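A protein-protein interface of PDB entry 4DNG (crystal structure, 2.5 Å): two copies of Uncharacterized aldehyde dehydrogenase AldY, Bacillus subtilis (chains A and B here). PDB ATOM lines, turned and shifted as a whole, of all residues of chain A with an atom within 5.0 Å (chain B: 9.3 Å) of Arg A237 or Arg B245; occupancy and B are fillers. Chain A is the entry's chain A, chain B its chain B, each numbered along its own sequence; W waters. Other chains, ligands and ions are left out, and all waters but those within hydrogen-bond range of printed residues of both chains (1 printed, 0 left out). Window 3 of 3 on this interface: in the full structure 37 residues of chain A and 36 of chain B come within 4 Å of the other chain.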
ATOM      1  N   THR A 233     -16.989  22.144  -0.953  1.00  0.00           N
ATOM      2  CA  THR A 233     -16.859  20.757  -1.404  1.00  0.00           C
ATOM      3  C   THR A 233     -18.123  19.883  -1.221  1.00  0.00           C
ATOM      4  O   THR A 233     -18.468  19.097  -2.107  1.00  0.00           O
ATOM      5  CB  THR A 233     -15.637  20.150  -0.727  1.00  0.00           C
ATOM      6  OG1 THR A 233     -14.526  20.987  -1.041  1.00  0.00           O
ATOM      7  CG2 THR A 233     -15.343  18.713  -1.198  1.00  0.00           C
ATOM      8  N   ALA A 234     -18.832  20.058  -0.107  1.00  0.00           N
ATOM      9  CA  ALA A 234     -19.960  19.189   0.237  1.00  0.00           C
ATOM     10  C   ALA A 234     -21.134  19.399  -0.710  1.00  0.00           C
ATOM     11  O   ALA A 234     -21.785  18.439  -1.126  1.00  0.00           O
ATOM     12  CB  ALA A 234     -20.372  19.393   1.700  1.00  0.00           C
ATOM     13  N   VAL A 235     -21.392  20.658  -1.053  1.00  0.00           N
ATOM     14  CA  VAL A 235     -22.332  21.016  -2.109  1.00  0.00           C
ATOM     15  C   VAL A 235     -21.810  20.492  -3.481  1.00  0.00           C
ATOM     16  O   VAL A 235     -22.561  19.888  -4.269  1.00  0.00           O
ATOM     17  CB  VAL A 235     -22.595  22.544  -2.093  1.00  0.00           C
ATOM     18  CG1 VAL A 235     -23.659  22.952  -3.112  1.00  0.00           C
ATOM     19  CG2 VAL A 235     -23.024  22.993  -0.689  1.00  0.00           C
ATOM     20  N   GLY A 236     -20.516  20.673  -3.742  1.00  0.00           N
ATOM     21  CA  GLY A 236     -19.867  20.044  -4.900  1.00  0.00           C
ATOM     22  C   GLY A 236     -20.193  18.558  -5.044  1.00  0.00           C
ATOM     23  O   GLY A 236     -20.632  18.115  -6.105  1.00  0.00           O
ATOM     24  N   ARG A 237     -20.002  17.777  -3.979  1.00  0.00           N
ATOM     25  CA  ARG A 237     -20.268  16.350  -4.076  1.00  0.00           C
ATOM     26  C   ARG A 237     -21.736  16.109  -4.415  1.00  0.00           C
ATOM     27  O   ARG A 237     -22.072  15.209  -5.192  1.00  0.00           O
ATOM     28  CB  ARG A 237     -19.861  15.621  -2.785  1.00  0.00           C
ATOM     29  CG  ARG A 237     -18.396  15.838  -2.400  1.00  0.00           C
ATOM     30  CD  ARG A 237     -17.940  14.990  -1.214  1.00  0.00           C
ATOM     31  NE  ARG A 237     -16.612  14.530  -1.549  1.00  0.00           N
ATOM     32  CZ  ARG A 237     -15.496  14.957  -0.991  1.00  0.00           C
ATOM     33  NH1 ARG A 237     -14.348  14.482  -1.429  1.00  0.00           N
ATOM     34  NH2 ARG A 237     -15.532  15.821   0.005  1.00  0.00           N
ATOM     35  N   HIS A 238     -22.604  16.935  -3.837  1.00  0.00           N
ATOM     36  CA  HIS A 238     -24.044  16.861  -4.061  1.00  0.00           C
ATOM     37  C   HIS A 238     -24.367  17.167  -5.511  1.00  0.00           C
ATOM     38  O   HIS A 238     -25.202  16.501  -6.128  1.00  0.00           O
ATOM     39  CB  HIS A 238     -24.728  17.831  -3.090  1.00  0.00           C
ATOM     40  CG  HIS A 238     -26.246  17.780  -3.080  1.00  0.00           C
ATOM     41  ND1 HIS A 238     -26.938  16.818  -2.447  1.00  0.00           N
ATOM     42  CD2 HIS A 238     -27.197  18.673  -3.597  1.00  0.00           C
ATOM     43  CE1 HIS A 238     -28.257  17.048  -2.598  1.00  0.00           C
ATOM     44  NE2 HIS A 238     -28.409  18.195  -3.286  1.00  0.00           N
ATOM     45  N   ILE A 239     -23.708  18.165  -6.082  1.00  0.00           N
ATOM     46  CA  ILE A 239     -23.871  18.443  -7.502  1.00  0.00           C
ATOM     47  C   ILE A 239     -23.306  17.295  -8.352  1.00  0.00           C
ATOM     48  O   ILE A 239     -23.953  16.819  -9.285  1.00  0.00           O
ATOM     49  CB  ILE A 239     -23.179  19.757  -7.886  1.00  0.00           C
ATOM     50  CG1 ILE A 239     -23.903  20.895  -7.201  1.00  0.00           C
ATOM     51  CG2 ILE A 239     -23.130  19.914  -9.419  1.00  0.00           C
ATOM     52  CD1 ILE A 239     -23.111  22.174  -7.143  1.00  0.00           C
ATOM     53  N   GLY A 240     -22.110  16.839  -8.006  1.00  0.00           N
ATOM     54  CA  GLY A 240     -21.442  15.775  -8.765  1.00  0.00           C
ATOM     55  C   GLY A 240     -22.269  14.515  -8.888  1.00  0.00           C
ATOM     56  O   GLY A 240     -22.277  13.846  -9.920  1.00  0.00           O
ATOM     57  N   GLU A 241     -22.989  14.198  -7.828  1.00  0.00           N
ATOM     58  CA  GLU A 241     -23.811  13.010  -7.826  1.00  0.00           C
ATOM     59  C   GLU A 241     -25.033  13.212  -8.727  1.00  0.00           C
ATOM     60  O   GLU A 241     -25.361  12.354  -9.554  1.00  0.00           O
ATOM     61  CB  GLU A 241     -24.166  12.693  -6.383  1.00  0.00           C
ATOM     62  CG  GLU A 241     -25.417  11.887  -6.099  1.00  0.00           C
ATOM     63  CD  GLU A 241     -25.921  12.169  -4.699  1.00  0.00           C
ATOM     64  OE1 GLU A 241     -25.994  11.242  -3.870  1.00  0.00           O
ATOM     65  OE2 GLU A 241     -26.207  13.354  -4.418  1.00  0.00           O
ATOM     66  N   TYR A 407      -7.678  18.943  -1.845  1.00  0.00           N
ATOM     67  CA  TYR A 407      -7.463  19.184  -3.279  1.00  0.00           C
ATOM     68  C   TYR A 407      -6.666  20.468  -3.481  1.00  0.00           C
ATOM     69  O   TYR A 407      -6.635  21.343  -2.607  1.00  0.00           O
ATOM     70  CB  TYR A 407      -8.786  19.253  -4.065  1.00  0.00           C
ATOM     71  CG  TYR A 407      -9.632  18.004  -3.953  1.00  0.00           C
ATOM     72  CD1 TYR A 407      -9.356  16.875  -4.730  1.00  0.00           C
ATOM     73  CD2 TYR A 407     -10.699  17.946  -3.055  1.00  0.00           C
ATOM     74  CE1 TYR A 407     -10.120  15.723  -4.613  1.00  0.00           C
ATOM     75  CE2 TYR A 407     -11.467  16.801  -2.932  1.00  0.00           C
ATOM     76  CZ  TYR A 407     -11.175  15.694  -3.711  1.00  0.00           C
ATOM     77  OH  TYR A 407     -11.946  14.561  -3.586  1.00  0.00           O
ATOM     78  N   ASP B 216     -18.712  -1.937  -5.288  1.00  0.00           N
ATOM     79  CA  ASP B 216     -18.289  -0.806  -6.157  1.00  0.00           C
ATOM     80  C   ASP B 216     -16.778  -0.530  -6.078  1.00  0.00           C
ATOM     81  O   ASP B 216     -16.324   0.567  -6.423  1.00  0.00           O
ATOM     82  CB  ASP B 216     -19.049   0.495  -5.811  1.00  0.00           C
ATOM     83  CG  ASP B 216     -20.579   0.394  -6.019  1.00  0.00           C
ATOM     84  OD1 ASP B 216     -21.054  -0.084  -7.069  1.00  0.00           O
ATOM     85  OD2 ASP B 216     -21.321   0.847  -5.121  1.00  0.00           O
ATOM     86  N   LEU B 219     -14.998   1.716  -8.517  1.00  0.00           N
ATOM     87  CA  LEU B 219     -15.498   3.082  -8.639  1.00  0.00           C
ATOM     88  C   LEU B 219     -15.181   3.908  -7.416  1.00  0.00           C
ATOM     89  O   LEU B 219     -14.981   5.122  -7.510  1.00  0.00           O
ATOM     90  CB  LEU B 219     -17.011   3.030  -8.768  1.00  0.00           C
ATOM     91  CG  LEU B 219     -17.518   2.097  -9.866  1.00  0.00           C
ATOM     92  CD1 LEU B 219     -19.019   1.944  -9.748  1.00  0.00           C
ATOM     93  CD2 LEU B 219     -17.111   2.642 -11.227  1.00  0.00           C
ATOM     94  N   THR B 220     -15.161   3.236  -6.269  1.00  0.00           N
ATOM     95  CA  THR B 220     -15.097   3.869  -4.957  1.00  0.00           C
ATOM     96  C   THR B 220     -13.683   4.222  -4.491  1.00  0.00           C
ATOM     97  O   THR B 220     -13.504   5.183  -3.754  1.00  0.00           O
ATOM     98  CB  THR B 220     -15.754   2.944  -3.922  1.00  0.00           C
ATOM     99  OG1 THR B 220     -17.160   3.194  -3.926  1.00  0.00           O
ATOM    100  CG2 THR B 220     -15.187   3.166  -2.525  1.00  0.00           C
ATOM    101  N   PRO B 222     -10.193   5.707  -3.879  1.00  0.00           N
ATOM    102  CA  PRO B 222      -9.715   7.079  -4.122  1.00  0.00           C
ATOM    103  C   PRO B 222      -8.511   7.167  -5.059  1.00  0.00           C
ATOM    104  O   PRO B 222      -8.264   8.224  -5.637  1.00  0.00           O
ATOM    105  CB  PRO B 222      -9.330   7.579  -2.713  1.00  0.00           C
ATOM    106  CG  PRO B 222      -9.151   6.352  -1.888  1.00  0.00           C
ATOM    107  CD  PRO B 222     -10.125   5.351  -2.448  1.00  0.00           C
ATOM    108  N   ARG B 237     -25.546   5.419 -15.372  1.00  0.00           N
ATOM    109  CA  ARG B 237     -26.141   6.293 -14.359  1.00  0.00           C
ATOM    110  C   ARG B 237     -25.564   6.011 -12.987  1.00  0.00           C
ATOM    111  O   ARG B 237     -25.296   6.929 -12.217  1.00  0.00           O
ATOM    112  CB  ARG B 237     -27.662   6.129 -14.317  1.00  0.00           C
ATOM    113  CG  ARG B 237     -28.391   6.997 -15.323  1.00  0.00           C
ATOM    114  CD  ARG B 237     -29.880   7.051 -15.037  1.00  0.00           C
ATOM    115  NE  ARG B 237     -30.633   6.239 -15.984  1.00  0.00           N
ATOM    116  CZ  ARG B 237     -31.054   6.668 -17.175  1.00  0.00           C
ATOM    117  NH1 ARG B 237     -31.733   5.842 -17.965  1.00  0.00           N
ATOM    118  NH2 ARG B 237     -30.796   7.916 -17.578  1.00  0.00           N
ATOM    119  N   HIS B 238     -25.386   4.730 -12.685  1.00  0.00           N
ATOM    120  CA  HIS B 238     -24.846   4.310 -11.413  1.00  0.00           C
ATOM    121  C   HIS B 238     -23.396   4.735 -11.298  1.00  0.00           C
ATOM    122  O   HIS B 238     -23.000   5.320 -10.290  1.00  0.00           O
ATOM    123  CB  HIS B 238     -24.997   2.801 -11.272  1.00  0.00           C
ATOM    124  CG  HIS B 238     -24.331   2.239 -10.044  1.00  0.00           C
ATOM    125  ND1 HIS B 238     -24.800   2.460  -8.801  1.00  0.00           N
ATOM    126  CD2 HIS B 238     -23.196   1.449  -9.902  1.00  0.00           C
ATOM    127  CE1 HIS B 238     -24.013   1.843  -7.909  1.00  0.00           C
ATOM    128  NE2 HIS B 238     -23.038   1.209  -8.585  1.00  0.00           N
ATOM    129  N   ILE B 239     -22.589   4.457 -12.324  1.00  0.00           N
ATOM    130  CA  ILE B 239     -21.184   4.867 -12.312  1.00  0.00           C
ATOM    131  C   ILE B 239     -21.043   6.400 -12.259  1.00  0.00           C
ATOM    132  O   ILE B 239     -20.258   6.942 -11.458  1.00  0.00           O
ATOM    133  CB  ILE B 239     -20.426   4.274 -13.512  1.00  0.00           C
ATOM    134  CG1 ILE B 239     -20.213   2.781 -13.290  1.00  0.00           C
ATOM    135  CG2 ILE B 239     -19.083   4.971 -13.719  1.00  0.00           C
ATOM    136  CD1 ILE B 239     -20.508   1.976 -14.518  1.00  0.00           C
ATOM    137  N   GLY B 240     -21.833   7.080 -13.087  1.00  0.00           N
ATOM    138  CA  GLY B 240     -21.824   8.542 -13.190  1.00  0.00           C
ATOM    139  C   GLY B 240     -22.111   9.235 -11.877  1.00  0.00           C
ATOM    140  O   GLY B 240     -21.534  10.275 -11.573  1.00  0.00           O
ATOM    141  N   GLU B 241     -22.983   8.642 -11.085  1.00  0.00           N
ATOM    142  CA  GLU B 241     -23.353   9.203  -9.803  1.00  0.00           C
ATOM    143  C   GLU B 241     -22.230   8.970  -8.787  1.00  0.00           C
ATOM    144  O   GLU B 241     -21.975   9.832  -7.958  1.00  0.00           O
ATOM    145  CB  GLU B 241     -24.672   8.581  -9.362  1.00  0.00           C
ATOM    146  CG  GLU B 241     -25.094   8.802  -7.919  1.00  0.00           C
ATOM    147  CD  GLU B 241     -26.054   7.718  -7.449  1.00  0.00           C
ATOM    148  OE1 GLU B 241     -25.632   6.841  -6.664  1.00  0.00           O
ATOM    149  OE2 GLU B 241     -27.222   7.728  -7.888  1.00  0.00           O
ATOM    150  N   ILE B 242     -21.546   7.826  -8.855  1.00  0.00           N
ATOM    151  CA  ILE B 242     -20.456   7.541  -7.896  1.00  0.00           C
ATOM    152  C   ILE B 242     -19.238   8.395  -8.226  1.00  0.00           C
ATOM    153  O   ILE B 242     -18.657   9.021  -7.350  1.00  0.00           O
ATOM    154  CB  ILE B 242     -20.028   6.044  -7.836  1.00  0.00           C
ATOM    155  CG1 ILE B 242     -21.237   5.100  -7.696  1.00  0.00           C
ATOM    156  CG2 ILE B 242     -19.037   5.815  -6.704  1.00  0.00           C
ATOM    157  CD1 ILE B 242     -21.658   4.791  -6.274  1.00  0.00           C
ATOM    158  N   ALA B 243     -18.874   8.430  -9.498  1.00  0.00           N
ATOM    159  CA  ALA B 243     -17.712   9.186  -9.947  1.00  0.00           C
ATOM    160  C   ALA B 243     -17.866  10.705  -9.729  1.00  0.00           C
ATOM    161  O   ALA B 243     -16.974  11.352  -9.164  1.00  0.00           O
ATOM    162  CB  ALA B 243     -17.408   8.872 -11.408  1.00  0.00           C
ATOM    163  N   GLY B 244     -18.995  11.269 -10.156  1.00  0.00           N
ATOM    164  CA  GLY B 244     -19.244  12.712  -9.991  1.00  0.00           C
ATOM    165  C   GLY B 244     -19.063  13.152  -8.552  1.00  0.00           C
ATOM    166  O   GLY B 244     -18.605  14.240  -8.281  1.00  0.00           O
ATOM    167  N   ARG B 245     -19.396  12.257  -7.633  1.00  0.00           N
ATOM    168  CA  ARG B 245     -19.435  12.538  -6.213  1.00  0.00           C
ATOM    169  C   ARG B 245     -18.028  12.486  -5.627  1.00  0.00           C
ATOM    170  O   ARG B 245     -17.756  13.030  -4.570  1.00  0.00           O
ATOM    171  CB  ARG B 245     -20.305  11.455  -5.609  1.00  0.00           C
ATOM    172  CG  ARG B 245     -20.653  11.563  -4.151  1.00  0.00           C
ATOM    173  CD  ARG B 245     -22.021  10.928  -3.949  1.00  0.00           C
ATOM    174  NE  ARG B 245     -22.049   9.498  -4.235  1.00  0.00           N
ATOM    175  CZ  ARG B 245     -23.164   8.774  -4.295  1.00  0.00           C
ATOM    176  NH1 ARG B 245     -23.104   7.474  -4.557  1.00  0.00           N
ATOM    177  NH2 ARG B 245     -24.343   9.343  -4.085  1.00  0.00           N
ATOM    178  N   ALA B 246     -17.141  11.788  -6.312  1.00  0.00           N
ATOM    179  CA  ALA B 246     -15.739  11.751  -5.931  1.00  0.00           C
ATOM    180  C   ALA B 246     -14.889  12.711  -6.792  1.00  0.00           C
ATOM    181  O   ALA B 246     -13.692  12.813  -6.584  1.00  0.00           O
ATOM    182  CB  ALA B 246     -15.221  10.333  -6.028  1.00  0.00           C
ATOM    183  N   PHE B 247     -15.522  13.427  -7.727  1.00  0.00           N
ATOM    184  CA  PHE B 247     -14.835  14.323  -8.673  1.00  0.00           C
ATOM    185  C   PHE B 247     -13.818  13.608  -9.578  1.00  0.00           C
ATOM    186  O   PHE B 247     -12.812  14.189  -9.988  1.00  0.00           O
ATOM    187  CB  PHE B 247     -14.156  15.481  -7.948  1.00  0.00           C
ATOM    188  CG  PHE B 247     -15.015  16.138  -6.912  1.00  0.00           C
ATOM    189  CD1 PHE B 247     -16.263  16.690  -7.257  1.00  0.00           C
ATOM    190  CD2 PHE B 247     -14.568  16.235  -5.582  1.00  0.00           C
ATOM    191  CE1 PHE B 247     -17.042  17.307  -6.300  1.00  0.00           C
ATOM    192  CE2 PHE B 247     -15.343  16.865  -4.622  1.00  0.00           C
ATOM    193  CZ  PHE B 247     -16.582  17.400  -4.984  1.00  0.00           C
ATOM    194  N   LYS B 248     -14.088  12.349  -9.885  1.00  0.00           N
ATOM    195  CA  LYS B 248     -13.286  11.582 -10.834  1.00  0.00           C
ATOM    196  C   LYS B 248     -13.690  11.935 -12.256  1.00  0.00           C
ATOM    197  O   LYS B 248     -14.859  12.150 -12.550  1.00  0.00           O
ATOM    198  CB  LYS B 248     -13.504  10.071 -10.615  1.00  0.00           C
ATOM    199  CG  LYS B 248     -13.003   9.564  -9.276  1.00  0.00           C
ATOM    200  CD  LYS B 248     -13.210   8.063  -9.129  1.00  0.00           C
ATOM    201  CE  LYS B 248     -12.777   7.572  -7.746  1.00  0.00           C
ATOM    202  NZ  LYS B 248     -11.461   8.106  -7.277  1.00  0.00           N
ATOM    203  N   ARG B 249     -12.734  11.965 -13.163  1.00  0.00           N
ATOM    204  CA  ARG B 249     -13.084  12.169 -14.556  1.00  0.00           C
ATOM    205  C   ARG B 249     -13.717  10.857 -15.030  1.00  0.00           C
ATOM    206  O   ARG B 249     -13.399   9.799 -14.507  1.00  0.00           O
ATOM    207  CB  ARG B 249     -11.840  12.549 -15.366  1.00  0.00           C
ATOM    208  CG  ARG B 249     -12.139  13.306 -16.657  1.00  0.00           C
ATOM    209  CD  ARG B 249     -10.865  13.637 -17.417  1.00  0.00           C
ATOM    210  NE  ARG B 249     -10.025  14.586 -16.681  1.00  0.00           N
ATOM    211  CZ  ARG B 249      -8.771  14.891 -17.016  1.00  0.00           C
ATOM    212  NH1 ARG B 249      -8.195  14.313 -18.066  1.00  0.00           N
ATOM    213  NH2 ARG B 249      -8.090  15.771 -16.301  1.00  0.00           N
ATOM    214  N   MET B 250     -14.657  10.923 -15.962  1.00  0.00           N
ATOM    215  CA  MET B 250     -15.254   9.704 -16.501  1.00  0.00           C
ATOM    216  C   MET B 250     -15.215   9.676 -18.006  1.00  0.00           C
ATOM    217  O   MET B 250     -15.466  10.689 -18.655  1.00  0.00           O
ATOM    218  CB  MET B 250     -16.687   9.511 -16.029  1.00  0.00           C
ATOM    219  CG  MET B 250     -17.477  10.785 -15.878  1.00  0.00           C
ATOM    220  SD  MET B 250     -18.950  10.425 -14.910  1.00  0.00           S
ATOM    221  CE  MET B 250     -18.930  11.753 -13.714  1.00  0.00           C
HETATM  222  O   HOH W   1     -13.146  12.276  -3.259  1.00  0.00           O
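Water W1 lies within hydrogen-bond range of the side-chain hydroxyl of Tyr A407, the guanidinium group of Arg A237 and the backbone carbonyl oxygen of Ala B246.
The guanidinium group of Arg B245 lies within salt-bridge range of the side-chain carboxylate of Glu A241 (2.5 Å).
Glu A241 touches its own counterpart, Glu B241.
Phe B247 touches Thr A233.
Phe B247 touches Gly A236.
Arg B245 touches Arg A237 (O to NE, 3.6 Å).
Arg A237 touches Phe B247 (CG to CZ, 3.5 Å).
Gly A240 touches Gly B244.
N of Arg B245 touches C of Gly A240 (3.9 Å).
Glu B241 touches Glu A241 (CG to CG, 3.6 Å).
Tyr A407 touches Ala B246.
CD2 of Phe B247 touches OH of Tyr A407 (3.7 Å).
Arg A237 touches two residues of chain B.
Of the printed residues of chain A, Arg B245 touches Arg A237 (3.6 Å), Gly A240 (3.9 Å) and Glu A241 (2.5 Å).
Of the printed residues of chain B, Thr A233 touches Phe B247 (3.8 Å).
Printed residues of chain A within 4 Å of Glu B241: Glu A241 (3.6 Å).
Of the printed residues of chain A, Gly B244 touches Gly A240.
Met B250 touches none of the printed residues of chain A.
The nearest printed residue of chain B that does not touch Tyr A407 is Arg B245 (6.1 Å).
NH1 of Arg A237 is in hydrogen-bond range of OH of Tyr A407 (3.2 Å).
The side-chain carboxylate (OE1) of Glu B241 lies within salt-bridge range of the guanidinium group (NH1) of Arg B245 (3.4 Å).
Printed residues of chain A that touch a printed residue of chain B: Thr A233, Gly A236, Arg A237, Gly A240, Glu A241 and Tyr A407.
Of the 18 printed residues of chain B, 5 touch a printed residue of chain A.
Printed residues of chain B that touch a printed residue of chain A: Glu B241, Gly B244, Arg B245, Ala B246 and Phe B247.
Hydrophobic or aromatic side chains of chain B that line the printed part of chain A: Phe B247.
Among the printed residues, Asp or Glu carboxylates within 4 Å of a Lys or Arg side-chain nitrogen of the other chain: Glu A241 with Arg B245 (2.5 Å).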
